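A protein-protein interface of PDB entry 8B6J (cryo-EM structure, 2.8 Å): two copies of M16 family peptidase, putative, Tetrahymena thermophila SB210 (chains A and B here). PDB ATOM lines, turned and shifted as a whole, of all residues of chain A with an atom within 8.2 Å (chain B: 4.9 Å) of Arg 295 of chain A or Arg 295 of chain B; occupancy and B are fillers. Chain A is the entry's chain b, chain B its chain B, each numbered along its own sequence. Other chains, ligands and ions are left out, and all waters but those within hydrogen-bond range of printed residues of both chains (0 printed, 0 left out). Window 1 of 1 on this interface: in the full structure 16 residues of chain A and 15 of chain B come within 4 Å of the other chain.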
ATOM      1  N   THR A 210     -21.647   0.842  -2.647  1.00  0.00           N
ATOM      2  CA  THR A 210     -21.302  -0.161  -1.646  1.00  0.00           C
ATOM      3  C   THR A 210     -22.484  -0.455  -0.732  1.00  0.00           C
ATOM      4  O   THR A 210     -22.740  -1.614  -0.387  1.00  0.00           O
ATOM      5  CB  THR A 210     -20.106   0.315  -0.824  1.00  0.00           C
ATOM      6  OG1 THR A 210     -18.996   0.569  -1.692  1.00  0.00           O
ATOM      7  CG2 THR A 210     -19.714  -0.729   0.207  1.00  0.00           C
ATOM      8  N   GLY A 291     -23.513  -4.316   3.773  1.00  0.00           N
ATOM      9  CA  GLY A 291     -22.360  -3.653   4.350  1.00  0.00           C
ATOM     10  C   GLY A 291     -21.040  -4.038   3.713  1.00  0.00           C
ATOM     11  O   GLY A 291     -20.180  -4.630   4.370  1.00  0.00           O
ATOM     12  N   GLY A 292     -20.861  -3.708   2.436  1.00  0.00           N
ATOM     13  CA  GLY A 292     -19.624  -4.002   1.746  1.00  0.00           C
ATOM     14  C   GLY A 292     -18.528  -3.008   2.082  1.00  0.00           C
ATOM     15  O   GLY A 292     -18.710  -2.062   2.847  1.00  0.00           O
ATOM     16  N   GLU A 293     -17.356  -3.241   1.492  1.00  0.00           N
ATOM     17  CA  GLU A 293     -16.216  -2.356   1.672  1.00  0.00           C
ATOM     18  C   GLU A 293     -15.550  -2.095   0.329  1.00  0.00           C
ATOM     19  O   GLU A 293     -15.566  -2.944  -0.565  1.00  0.00           O
ATOM     20  CB  GLU A 293     -15.191  -2.936   2.654  1.00  0.00           C
ATOM     21  CG  GLU A 293     -14.568  -4.243   2.208  1.00  0.00           C
ATOM     22  CD  GLU A 293     -13.489  -4.723   3.158  1.00  0.00           C
ATOM     23  OE1 GLU A 293     -13.166  -3.987   4.112  1.00  0.00           O
ATOM     24  OE2 GLU A 293     -12.962  -5.837   2.949  1.00  0.00           O
ATOM     25  N   VAL A 294     -14.963  -0.907   0.199  1.00  0.00           N
ATOM     26  CA  VAL A 294     -14.248  -0.494  -1.002  1.00  0.00           C
ATOM     27  C   VAL A 294     -12.932   0.141  -0.579  1.00  0.00           C
ATOM     28  O   VAL A 294     -12.904   0.961   0.346  1.00  0.00           O
ATOM     29  CB  VAL A 294     -15.075   0.488  -1.850  1.00  0.00           C
ATOM     30  CG1 VAL A 294     -14.225   1.077  -2.964  1.00  0.00           C
ATOM     31  CG2 VAL A 294     -16.292  -0.209  -2.423  1.00  0.00           C
ATOM     32  N   ARG A 295     -11.847  -0.236  -1.253  1.00  0.00           N
ATOM     33  CA  ARG A 295     -10.504   0.243  -0.920  1.00  0.00           C
ATOM     34  C   ARG A 295      -9.797   0.569  -2.232  1.00  0.00           C
ATOM     35  O   ARG A 295      -9.349  -0.336  -2.942  1.00  0.00           O
ATOM     36  CB  ARG A 295      -9.733  -0.801  -0.119  1.00  0.00           C
ATOM     37  CG  ARG A 295     -10.476  -1.321   1.108  1.00  0.00           C
ATOM     38  CD  ARG A 295     -10.030  -2.721   1.485  1.00  0.00           C
ATOM     39  NE  ARG A 295      -8.759  -2.726   2.197  1.00  0.00           N
ATOM     40  CZ  ARG A 295      -8.635  -2.684   3.517  1.00  0.00           C
ATOM     41  NH1 ARG A 295      -9.692  -2.612   4.311  1.00  0.00           N
ATOM     42  NH2 ARG A 295      -7.420  -2.715   4.055  1.00  0.00           N
ATOM     43  N   ASN A 296      -9.695   1.857  -2.550  1.00  0.00           N
ATOM     44  CA  ASN A 296      -9.141   2.311  -3.820  1.00  0.00           C
ATOM     45  C   ASN A 296      -7.724   2.831  -3.625  1.00  0.00           C
ATOM     46  O   ASN A 296      -7.491   3.715  -2.793  1.00  0.00           O
ATOM     47  CB  ASN A 296     -10.014   3.409  -4.431  1.00  0.00           C
ATOM     48  CG  ASN A 296     -11.469   3.008  -4.531  1.00  0.00           C
ATOM     49  OD1 ASN A 296     -11.803   1.827  -4.484  1.00  0.00           O
ATOM     50  ND2 ASN A 296     -12.346   3.994  -4.675  1.00  0.00           N
ATOM     51  N   LEU A 297      -6.785   2.285  -4.392  1.00  0.00           N
ATOM     52  CA  LEU A 297      -5.431   2.819  -4.462  1.00  0.00           C
ATOM     53  C   LEU A 297      -5.368   3.866  -5.566  1.00  0.00           C
ATOM     54  O   LEU A 297      -5.755   3.597  -6.707  1.00  0.00           O
ATOM     55  CB  LEU A 297      -4.415   1.710  -4.735  1.00  0.00           C
ATOM     56  CG  LEU A 297      -3.945   0.869  -3.548  1.00  0.00           C
ATOM     57  CD1 LEU A 297      -3.046  -0.253  -4.034  1.00  0.00           C
ATOM     58  CD2 LEU A 297      -3.216   1.726  -2.530  1.00  0.00           C
ATOM     59  N   THR A 298      -4.878   5.060  -5.223  1.00  0.00           N
ATOM     60  CA  THR A 298      -4.848   6.156  -6.182  1.00  0.00           C
ATOM     61  C   THR A 298      -3.551   6.957  -6.125  1.00  0.00           C
ATOM     62  O   THR A 298      -3.435   7.965  -6.832  1.00  0.00           O
ATOM     63  CB  THR A 298      -6.044   7.089  -5.950  1.00  0.00           C
ATOM     64  OG1 THR A 298      -7.230   6.309  -5.760  1.00  0.00           O
ATOM     65  CG2 THR A 298      -6.250   8.018  -7.140  1.00  0.00           C
ATOM     66  N   THR A 304      -8.946   9.486   2.174  1.00  0.00           N
ATOM     67  CA  THR A 304     -10.319   9.813   2.535  1.00  0.00           C
ATOM     68  C   THR A 304     -11.055   8.522   2.873  1.00  0.00           C
ATOM     69  O   THR A 304     -11.092   7.593   2.058  1.00  0.00           O
ATOM     70  CB  THR A 304     -11.025  10.549   1.397  1.00  0.00           C
ATOM     71  OG1 THR A 304     -10.259  11.700   1.020  1.00  0.00           O
ATOM     72  CG2 THR A 304     -12.417  10.990   1.823  1.00  0.00           C
ATOM     73  N   LEU A 376      -8.503   6.300  10.942  1.00  0.00           N
ATOM     74  CA  LEU A 376      -9.618   5.362  11.024  1.00  0.00           C
ATOM     75  C   LEU A 376      -9.991   5.087  12.476  1.00  0.00           C
ATOM     76  O   LEU A 376     -11.172   5.119  12.847  1.00  0.00           O
ATOM     77  CB  LEU A 376      -9.251   4.062  10.307  1.00  0.00           C
ATOM     78  CG  LEU A 376     -10.395   3.244   9.706  1.00  0.00           C
ATOM     79  CD1 LEU A 376      -9.859   1.938   9.146  1.00  0.00           C
ATOM     80  CD2 LEU A 376     -11.487   2.981  10.725  1.00  0.00           C
ATOM     81  N   PHE A 461     -17.918   0.660   4.734  1.00  0.00           N
ATOM     82  CA  PHE A 461     -16.590   1.245   4.870  1.00  0.00           C
ATOM     83  C   PHE A 461     -15.996   1.466   3.488  1.00  0.00           C
ATOM     84  O   PHE A 461     -15.847   0.516   2.714  1.00  0.00           O
ATOM     85  CB  PHE A 461     -15.690   0.335   5.710  1.00  0.00           C
ATOM     86  CG  PHE A 461     -14.237   0.699   5.659  1.00  0.00           C
ATOM     87  CD1 PHE A 461     -13.757   1.792   6.357  1.00  0.00           C
ATOM     88  CD2 PHE A 461     -13.346  -0.063   4.924  1.00  0.00           C
ATOM     89  CE1 PHE A 461     -12.419   2.126   6.315  1.00  0.00           C
ATOM     90  CE2 PHE A 461     -12.006   0.265   4.879  1.00  0.00           C
ATOM     91  CZ  PHE A 461     -11.543   1.361   5.575  1.00  0.00           C
ATOM     92  N   VAL A 462     -15.649   2.713   3.183  1.00  0.00           N
ATOM     93  CA  VAL A 462     -15.048   3.079   1.905  1.00  0.00           C
ATOM     94  C   VAL A 462     -13.750   3.817   2.185  1.00  0.00           C
ATOM     95  O   VAL A 462     -13.713   4.707   3.040  1.00  0.00           O
ATOM     96  CB  VAL A 462     -15.997   3.947   1.059  1.00  0.00           C
ATOM     97  CG1 VAL A 462     -15.358   4.292  -0.278  1.00  0.00           C
ATOM     98  CG2 VAL A 462     -17.316   3.233   0.857  1.00  0.00           C
ATOM     99  N   ALA A 463     -12.686   3.444   1.479  1.00  0.00           N
ATOM    100  CA  ALA A 463     -11.383   4.066   1.668  1.00  0.00           C
ATOM    101  C   ALA A 463     -10.744   4.353   0.319  1.00  0.00           C
ATOM    102  O   ALA A 463     -10.765   3.509  -0.580  1.00  0.00           O
ATOM    103  CB  ALA A 463     -10.458   3.173   2.503  1.00  0.00           C
ATOM    104  N   GLN A 464     -10.179   5.551   0.184  1.00  0.00           N
ATOM    105  CA  GLN A 464      -9.382   5.922  -0.974  1.00  0.00           C
ATOM    106  C   GLN A 464      -8.105   6.589  -0.490  1.00  0.00           C
ATOM    107  O   GLN A 464      -8.107   7.293   0.520  1.00  0.00           O
ATOM    108  CB  GLN A 464     -10.135   6.875  -1.906  1.00  0.00           C
ATOM    109  CG  GLN A 464     -11.502   6.382  -2.323  1.00  0.00           C
ATOM    110  CD  GLN A 464     -12.148   7.280  -3.356  1.00  0.00           C
ATOM    111  OE1 GLN A 464     -11.553   8.262  -3.799  1.00  0.00           O
ATOM    112  NE2 GLN A 464     -13.373   6.947  -3.746  1.00  0.00           N
ATOM    113  N   GLY A 465      -7.016   6.361  -1.204  1.00  0.00           N
ATOM    114  CA  GLY A 465      -5.756   6.983  -0.863  1.00  0.00           C
ATOM    115  C   GLY A 465      -4.588   6.108  -1.267  1.00  0.00           C
ATOM    116  O   GLY A 465      -4.748   5.087  -1.928  1.00  0.00           O
ATOM    117  N   GLN A 467      -2.298   4.538   0.820  1.00  0.00           N
ATOM    118  CA  GLN A 467      -2.041   3.393   1.686  1.00  0.00           C
ATOM    119  C   GLN A 467      -3.339   2.822   2.245  1.00  0.00           C
ATOM    120  O   GLN A 467      -3.433   2.481   3.426  1.00  0.00           O
ATOM    121  CB  GLN A 467      -1.090   3.772   2.816  1.00  0.00           C
ATOM    122  CG  GLN A 467       0.293   4.180   2.341  1.00  0.00           C
ATOM    123  CD  GLN A 467       1.269   4.372   3.481  1.00  0.00           C
ATOM    124  OE1 GLN A 467       0.915   4.214   4.648  1.00  0.00           O
ATOM    125  NE2 GLN A 467       2.508   4.711   3.148  1.00  0.00           N
ATOM    126  N   VAL A 468      -4.361   2.714   1.396  1.00  0.00           N
ATOM    127  CA  VAL A 468      -5.607   2.089   1.821  1.00  0.00           C
ATOM    128  C   VAL A 468      -5.396   0.605   2.089  1.00  0.00           C
ATOM    129  O   VAL A 468      -6.091   0.013   2.923  1.00  0.00           O
ATOM    130  CB  VAL A 468      -6.705   2.311   0.767  1.00  0.00           C
ATOM    131  CG1 VAL A 468      -6.857   3.788   0.465  1.00  0.00           C
ATOM    132  CG2 VAL A 468      -6.395   1.530  -0.496  1.00  0.00           C
ATOM    133  N   ASN A 469      -4.443  -0.018   1.392  1.00  0.00           N
ATOM    134  CA  ASN A 469      -4.219  -1.450   1.560  1.00  0.00           C
ATOM    135  C   ASN A 469      -3.828  -1.786   2.994  1.00  0.00           C
ATOM    136  O   ASN A 469      -4.293  -2.787   3.553  1.00  0.00           O
ATOM    137  CB  ASN A 469      -3.144  -1.925   0.583  1.00  0.00           C
ATOM    138  CG  ASN A 469      -1.866  -1.116   0.684  1.00  0.00           C
ATOM    139  OD1 ASN A 469      -1.455  -0.715   1.771  1.00  0.00           O
ATOM    140  ND2 ASN A 469      -1.235  -0.864  -0.456  1.00  0.00           N
ATOM    141  N   ALA A 470      -2.977  -0.964   3.607  1.00  0.00           N
ATOM    142  CA  ALA A 470      -2.523  -1.196   4.978  1.00  0.00           C
ATOM    143  C   ALA A 470      -3.544  -0.613   5.957  1.00  0.00           C
ATOM    144  O   ALA A 470      -3.301   0.367   6.664  1.00  0.00           O
ATOM    145  CB  ALA A 470      -1.140  -0.598   5.188  1.00  0.00           C
ATOM    146  N   LEU A 471      -4.710  -1.242   5.987  1.00  0.00           N
ATOM    147  CA  LEU A 471      -5.785  -0.882   6.896  1.00  0.00           C
ATOM    148  C   LEU A 471      -6.360  -2.152   7.499  1.00  0.00           C
ATOM    149  O   LEU A 471      -6.208  -3.239   6.931  1.00  0.00           O
ATOM    150  CB  LEU A 471      -6.895  -0.094   6.187  1.00  0.00           C
ATOM    151  CG  LEU A 471      -6.553   1.330   5.749  1.00  0.00           C
ATOM    152  CD1 LEU A 471      -7.688   1.923   4.934  1.00  0.00           C
ATOM    153  CD2 LEU A 471      -6.253   2.204   6.954  1.00  0.00           C
ATOM    154  N   PRO A 472      -7.019  -2.052   8.653  1.00  0.00           N
ATOM    155  CA  PRO A 472      -7.615  -3.247   9.259  1.00  0.00           C
ATOM    156  C   PRO A 472      -8.667  -3.867   8.352  1.00  0.00           C
ATOM    157  O   PRO A 472      -9.349  -3.180   7.590  1.00  0.00           O
ATOM    158  CB  PRO A 472      -8.236  -2.719  10.557  1.00  0.00           C
ATOM    159  CG  PRO A 472      -7.526  -1.447  10.838  1.00  0.00           C
ATOM    160  CD  PRO A 472      -7.197  -0.863   9.501  1.00  0.00           C
ATOM    161  N   THR A 473      -8.790  -5.188   8.443  1.00  0.00           N
ATOM    162  CA  THR A 473      -9.776  -5.904   7.654  1.00  0.00           C
ATOM    163  C   THR A 473     -11.188  -5.536   8.109  1.00  0.00           C
ATOM    164  O   THR A 473     -11.395  -4.901   9.145  1.00  0.00           O
ATOM    165  CB  THR A 473      -9.564  -7.413   7.770  1.00  0.00           C
ATOM    166  OG1 THR A 473      -9.697  -7.813   9.140  1.00  0.00           O
ATOM    167  CG2 THR A 473      -8.184  -7.798   7.263  1.00  0.00           C
ATOM    168  N   TYR A 474     -12.174  -5.955   7.311  1.00  0.00           N
ATOM    169  CA  TYR A 474     -13.564  -5.642   7.627  1.00  0.00           C
ATOM    170  C   TYR A 474     -13.957  -6.205   8.986  1.00  0.00           C
ATOM    171  O   TYR A 474     -14.630  -5.532   9.778  1.00  0.00           O
ATOM    172  CB  TYR A 474     -14.475  -6.189   6.530  1.00  0.00           C
ATOM    173  CG  TYR A 474     -15.917  -5.750   6.637  1.00  0.00           C
ATOM    174  CD1 TYR A 474     -16.329  -4.525   6.135  1.00  0.00           C
ATOM    175  CD2 TYR A 474     -16.869  -6.566   7.230  1.00  0.00           C
ATOM    176  CE1 TYR A 474     -17.644  -4.122   6.225  1.00  0.00           C
ATOM    177  CE2 TYR A 474     -18.186  -6.171   7.326  1.00  0.00           C
ATOM    178  CZ  TYR A 474     -18.568  -4.949   6.822  1.00  0.00           C
ATOM    179  OH  TYR A 474     -19.881  -4.551   6.915  1.00  0.00           O
ATOM    180  N   ASP A 475     -13.542  -7.439   9.278  1.00  0.00           N
ATOM    181  CA  ASP A 475     -13.832  -8.024  10.581  1.00  0.00           C
ATOM    182  C   ASP A 475     -13.178  -7.220  11.697  1.00  0.00           C
ATOM    183  O   ASP A 475     -13.762  -7.047  12.772  1.00  0.00           O
ATOM    184  CB  ASP A 475     -13.362  -9.478  10.618  1.00  0.00           C
ATOM    185  CG  ASP A 475     -13.777 -10.194  11.890  1.00  0.00           C
ATOM    186  OD1 ASP A 475     -14.451  -9.570  12.737  1.00  0.00           O
ATOM    187  OD2 ASP A 475     -13.431 -11.385  12.042  1.00  0.00           O
ATOM    188  N   ILE A 477     -12.586  -3.987  11.652  1.00  0.00           N
ATOM    189  CA  ILE A 477     -13.384  -2.775  11.818  1.00  0.00           C
ATOM    190  C   ILE A 477     -14.647  -3.078  12.612  1.00  0.00           C
ATOM    191  O   ILE A 477     -15.029  -2.322  13.514  1.00  0.00           O
ATOM    192  CB  ILE A 477     -13.716  -2.161  10.445  1.00  0.00           C
ATOM    193  CG1 ILE A 477     -12.435  -1.825   9.674  1.00  0.00           C
ATOM    194  CG2 ILE A 477     -14.576  -0.920  10.613  1.00  0.00           C
ATOM    195  CD1 ILE A 477     -11.545  -0.805  10.353  1.00  0.00           C
ATOM    196  N   GLU B 293      -5.049  -6.010   1.222  1.00  0.00           N
ATOM    197  CA  GLU B 293      -6.065  -6.241   0.207  1.00  0.00           C
ATOM    198  C   GLU B 293      -6.480  -4.912  -0.405  1.00  0.00           C
ATOM    199  O   GLU B 293      -6.481  -3.876   0.266  1.00  0.00           O
ATOM    200  CB  GLU B 293      -7.291  -6.958   0.784  1.00  0.00           C
ATOM    201  CG  GLU B 293      -7.969  -6.213   1.916  1.00  0.00           C
ATOM    202  CD  GLU B 293      -9.256  -6.877   2.354  1.00  0.00           C
ATOM    203  OE1 GLU B 293      -9.605  -7.928   1.779  1.00  0.00           O
ATOM    204  OE2 GLU B 293      -9.919  -6.349   3.270  1.00  0.00           O
ATOM    205  N   VAL B 294      -6.835  -4.951  -1.687  1.00  0.00           N
ATOM    206  CA  VAL B 294      -7.246  -3.770  -2.437  1.00  0.00           C
ATOM    207  C   VAL B 294      -8.506  -4.112  -3.218  1.00  0.00           C
ATOM    208  O   VAL B 294      -8.577  -5.166  -3.859  1.00  0.00           O
ATOM    209  CB  VAL B 294      -6.135  -3.284  -3.387  1.00  0.00           C
ATOM    210  CG1 VAL B 294      -6.605  -2.084  -4.186  1.00  0.00           C
ATOM    211  CG2 VAL B 294      -4.881  -2.947  -2.601  1.00  0.00           C
ATOM    212  N   ARG B 295      -9.499  -3.224  -3.164  1.00  0.00           N
ATOM    213  CA  ARG B 295     -10.798  -3.452  -3.799  1.00  0.00           C
ATOM    214  C   ARG B 295     -11.211  -2.151  -4.482  1.00  0.00           C
ATOM    215  O   ARG B 295     -11.783  -1.266  -3.840  1.00  0.00           O
ATOM    216  CB  ARG B 295     -11.839  -3.895  -2.776  1.00  0.00           C
ATOM    217  CG  ARG B 295     -11.413  -5.084  -1.921  1.00  0.00           C
ATOM    218  CD  ARG B 295     -12.155  -5.117  -0.596  1.00  0.00           C
ATOM    219  NE  ARG B 295     -13.528  -5.587  -0.734  1.00  0.00           N
ATOM    220  CZ  ARG B 295     -13.928  -6.831  -0.506  1.00  0.00           C
ATOM    221  NH1 ARG B 295     -13.079  -7.777  -0.135  1.00  0.00           N
ATOM    222  NH2 ARG B 295     -15.214  -7.135  -0.651  1.00  0.00           N
ATOM    223  N   ASN B 296     -10.928  -2.042  -5.777  1.00  0.00           N
ATOM    224  CA  ASN B 296     -11.165  -0.818  -6.532  1.00  0.00           C
ATOM    225  C   ASN B 296     -12.437  -0.948  -7.359  1.00  0.00           C
ATOM    226  O   ASN B 296     -12.588  -1.903  -8.127  1.00  0.00           O
ATOM    227  CB  ASN B 296      -9.985  -0.511  -7.455  1.00  0.00           C
ATOM    228  CG  ASN B 296      -8.650  -0.640  -6.755  1.00  0.00           C
ATOM    229  OD1 ASN B 296      -8.553  -0.464  -5.544  1.00  0.00           O
ATOM    230  ND2 ASN B 296      -7.611  -0.949  -7.519  1.00  0.00           N
ATOM    231  N   LEU B 297     -13.343   0.015  -7.205  1.00  0.00           N
ATOM    232  CA  LEU B 297     -14.538   0.100  -8.038  1.00  0.00           C
ATOM    233  C   LEU B 297     -14.188   0.895  -9.290  1.00  0.00           C
ATOM    234  O   LEU B 297     -13.882   2.089  -9.209  1.00  0.00           O
ATOM    235  CB  LEU B 297     -15.690   0.754  -7.279  1.00  0.00           C
ATOM    236  CG  LEU B 297     -16.583  -0.164  -6.443  1.00  0.00           C
ATOM    237  CD1 LEU B 297     -17.564   0.658  -5.629  1.00  0.00           C
ATOM    238  CD2 LEU B 297     -17.327  -1.150  -7.327  1.00  0.00           C
ATOM    239  N   PHE B 461      -4.786  -9.967  -1.765  1.00  0.00           N
ATOM    240  CA  PHE B 461      -5.966 -10.011  -2.616  1.00  0.00           C
ATOM    241  C   PHE B 461      -6.184  -8.651  -3.260  1.00  0.00           C
ATOM    242  O   PHE B 461      -6.197  -7.628  -2.568  1.00  0.00           O
ATOM    243  CB  PHE B 461      -7.194 -10.422  -1.798  1.00  0.00           C
ATOM    244  CG  PHE B 461      -8.456 -10.522  -2.601  1.00  0.00           C
ATOM    245  CD1 PHE B 461      -8.625 -11.534  -3.528  1.00  0.00           C
ATOM    246  CD2 PHE B 461      -9.481  -9.612  -2.417  1.00  0.00           C
ATOM    247  CE1 PHE B 461      -9.786 -11.630  -4.265  1.00  0.00           C
ATOM    248  CE2 PHE B 461     -10.647  -9.703  -3.150  1.00  0.00           C
ATOM    249  CZ  PHE B 461     -10.798 -10.714  -4.075  1.00  0.00           C
ATOM    250  N   ALA B 463      -8.744  -6.720  -6.320  1.00  0.00           N
ATOM    251  CA  ALA B 463      -9.940  -6.870  -7.139  1.00  0.00           C
ATOM    252  C   ALA B 463     -10.305  -5.530  -7.754  1.00  0.00           C
ATOM    253  O   ALA B 463     -10.464  -4.539  -7.035  1.00  0.00           O
ATOM    254  CB  ALA B 463     -11.108  -7.407  -6.307  1.00  0.00           C
ATOM    255  N   VAL B 468     -16.956  -5.321  -7.316  1.00  0.00           N
ATOM    256  CA  VAL B 468     -16.017  -5.843  -6.332  1.00  0.00           C
ATOM    257  C   VAL B 468     -16.457  -5.505  -4.914  1.00  0.00           C
ATOM    258  O   VAL B 468     -15.947  -6.092  -3.954  1.00  0.00           O
ATOM    259  CB  VAL B 468     -14.598  -5.306  -6.596  1.00  0.00           C
ATOM    260  CG1 VAL B 468     -14.112  -5.747  -7.965  1.00  0.00           C
ATOM    261  CG2 VAL B 468     -14.564  -3.790  -6.478  1.00  0.00           C
ATOM    262  N   ASN B 469     -17.392  -4.566  -4.758  1.00  0.00           N
ATOM    263  CA  ASN B 469     -17.875  -4.206  -3.430  1.00  0.00           C
ATOM    264  C   ASN B 469     -18.585  -5.361  -2.740  1.00  0.00           C
ATOM    265  O   ASN B 469     -18.746  -5.331  -1.516  1.00  0.00           O
ATOM    266  CB  ASN B 469     -18.814  -3.001  -3.525  1.00  0.00           C
ATOM    267  CG  ASN B 469     -19.952  -3.225  -4.499  1.00  0.00           C
ATOM    268  OD1 ASN B 469     -20.295  -4.361  -4.822  1.00  0.00           O
ATOM    269  ND2 ASN B 469     -20.542  -2.136  -4.977  1.00  0.00           N
ATOM    270  N   ALA B 470     -19.013  -6.373  -3.490  1.00  0.00           N
ATOM    271  CA  ALA B 470     -19.692  -7.544  -2.941  1.00  0.00           C
ATOM    272  C   ALA B 470     -18.799  -8.758  -3.179  1.00  0.00           C
ATOM    273  O   ALA B 470     -18.934  -9.461  -4.181  1.00  0.00           O
ATOM    274  CB  ALA B 470     -21.067  -7.728  -3.577  1.00  0.00           C
ATOM    275  N   LEU B 471     -17.885  -8.997  -2.249  1.00  0.00           N
ATOM    276  CA  LEU B 471     -16.994 -10.145  -2.282  1.00  0.00           C
ATOM    277  C   LEU B 471     -16.791 -10.643  -0.861  1.00  0.00           C
ATOM    278  O   LEU B 471     -17.008  -9.897   0.100  1.00  0.00           O
ATOM    279  CB  LEU B 471     -15.638  -9.795  -2.912  1.00  0.00           C
ATOM    280  CG  LEU B 471     -15.645  -9.490  -4.410  1.00  0.00           C
ATOM    281  CD1 LEU B 471     -14.265  -9.052  -4.866  1.00  0.00           C
ATOM    282  CD2 LEU B 471     -16.109 -10.697  -5.206  1.00  0.00           C
ATOM    283  N   PRO B 472     -16.379 -11.899  -0.695  1.00  0.00           N
ATOM    284  CA  PRO B 472     -16.152 -12.418   0.658  1.00  0.00           C
ATOM    285  C   PRO B 472     -15.108 -11.595   1.397  1.00  0.00           C
ATOM    286  O   PRO B 472     -14.126 -11.133   0.814  1.00  0.00           O
ATOM    287  CB  PRO B 472     -15.670 -13.852   0.414  1.00  0.00           C
ATOM    288  CG  PRO B 472     -16.153 -14.198  -0.950  1.00  0.00           C
ATOM    289  CD  PRO B 472     -16.131 -12.921  -1.725  1.00  0.00           C
ATOM    290  N   THR B 473     -15.328 -11.418   2.696  1.00  0.00           N
ATOM    291  CA  THR B 473     -14.399 -10.652   3.509  1.00  0.00           C
ATOM    292  C   THR B 473     -13.052 -11.361   3.592  1.00  0.00           C
ATOM    293  O   THR B 473     -12.942 -12.574   3.393  1.00  0.00           O
ATOM    294  CB  THR B 473     -14.962 -10.438   4.914  1.00  0.00           C
ATOM    295  OG1 THR B 473     -15.226 -11.707   5.524  1.00  0.00           O
ATOM    296  CG2 THR B 473     -16.247  -9.627   4.856  1.00  0.00           C
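The guanidinium group of Arg 295 of chain B is in salt-bridge range of the side-chain carboxylate of Glu 293 of chain B, 3.97 Å away. O of Gly 291 of chain A lies within hydrogen-bond range of OH of Tyr 474 of chain A (2.6 Å). The backbone NH (N) of Phe 461 of chain A lies within hydrogen-bond range of the backbone carbonyl oxygen (O) of Gly 292 of chain A, at 3.4 Å. O of Phe 461 of chain A sits at hydrogen-bond distance from N of Val 294 of chain A. NH2 of Arg 295 of chain A sits at hydrogen-bond distance from O of Asn 469 of chain A, at 3.2 Å. The backbone NH (N) of Gly 465 of chain A lies within hydrogen-bond range of the backbone carbonyl oxygen (O) of Asn 296 of chain A, at 3.1 Å.
Printed residues of chain B within 4 Å of Val 294 of chain A: Arg 295 (3.5 Å), Leu 297 (3.6 Å) and Asn 469 (3.9 Å). Of chain B, only Glu 293, Val 294, Arg 295 and Asn 296 come within 4 Å of Arg 295 of chain A. Of the printed residues of chain B, Leu 297 of chain A touches Val 294 and Asn 296. Of the printed residues of chain B, Tyr 474 of chain A touches Thr 473 (3.9 Å). Printed residues of chain A within 4 Å of Val 294 of chain B: Arg 295, Leu 297 and Asn 469. Arg 295 of chain B touches just these residues of chain A: Glu 293 (3.3 Å), Val 294 (3.5 Å), Arg 295 (2.8 Å) and Asn 296 (3.2 Å). The nearest printed residue of chain B that does not touch Arg 295 of chain A is Leu 297 of chain B (5.9 Å). The nearest residue of chain A that does not touch Arg 295 of chain B is Ala 463 of chain A (5.9 Å). The nearest printed residue of chain A that does not touch Glu 293 of chain B is Thr 473 of chain A (4.4 Å).
Of the 13 printed residues of chain B, 7 touch a printed residue of chain A. Hydrophobic or aromatic side chains of chain B within 4 Å of the printed part of chain A: Val 294 and Leu 297. Of the 26 printed residues of chain A, 9 touch a printed residue of chain B.
Among the printed residues, pairs that only touch across the chains: Thr 210 of chain A with Asn 469 of chain B, Gly 292 of chain A with Asn 469 of chain B, Glu 293 of chain A with Asn 469 of chain B, Val 294 of chain A with Arg 295 of chain B, Val 294 of chain A with Leu 297 of chain B, Val 294 of chain A with Asn 469 of chain B, Arg 295 of chain A with Val 294 of chain B, Asn 296 of chain A with Asn 296 of chain B, Asn 296 of chain A with Leu 297 of chain B, Leu 297 of chain A with Val 294 of chain B, Asn 469 of chain A with Glu 293 of chain B, Asn 469 of chain A with Val 294 of chain B and Tyr 474 of chain A with Thr 473 of chain B.
The side-chain carboxylate (OE2) of Glu 293 of chain B lies within salt-bridge range of the guanidinium group (NH1) of Arg 295 of chain A, 3.9 Å away. OE2 of Glu 293 of chain A is in salt-bridge range of NH1 of Arg 295 of chain B (3.6 Å). The backbone NH (N) of Arg 295 of chain A lies within hydrogen-bond range of the backbone carbonyl oxygen (O) of Arg 295 of chain B (2.8 Å). O of Arg 295 of chain B sits close to OD1 of Asn 296 of chain A (3.2 Å). O of Arg 295 of chain A sits close to OD1 of Asn 296 of chain B (2.7 Å). The side-chain amide oxygen (OD1) of Asn 296 of chain B is in hydrogen-bond range of the backbone NH (N) of Leu 297 of chain A (3.5 Å). The side-chain carboxylate (OE2) of Glu 293 of chain B sits close to the side-chain carboxylate (OE2) of Glu 293 of chain A, 3.1 Å away.
Glu 293 of chain A touches Asn 469 of chain B, and with the chains exchanged Asn 469 of chain A touches Glu 293 of chain B. Val 294 of chain A touches Arg 295 of chain B, and with the chains exchanged Arg 295 of chain A touches Val 294 of chain B. Val 294 of chain A touches Leu 297 of chain B, and with the chains exchanged Leu 297 of chain A touches Val 294 of chain B. Val 294 of chain A touches Asn 469 of chain B, and with the chains exchanged Asn 469 of chain A touches Val 294 of chain B.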
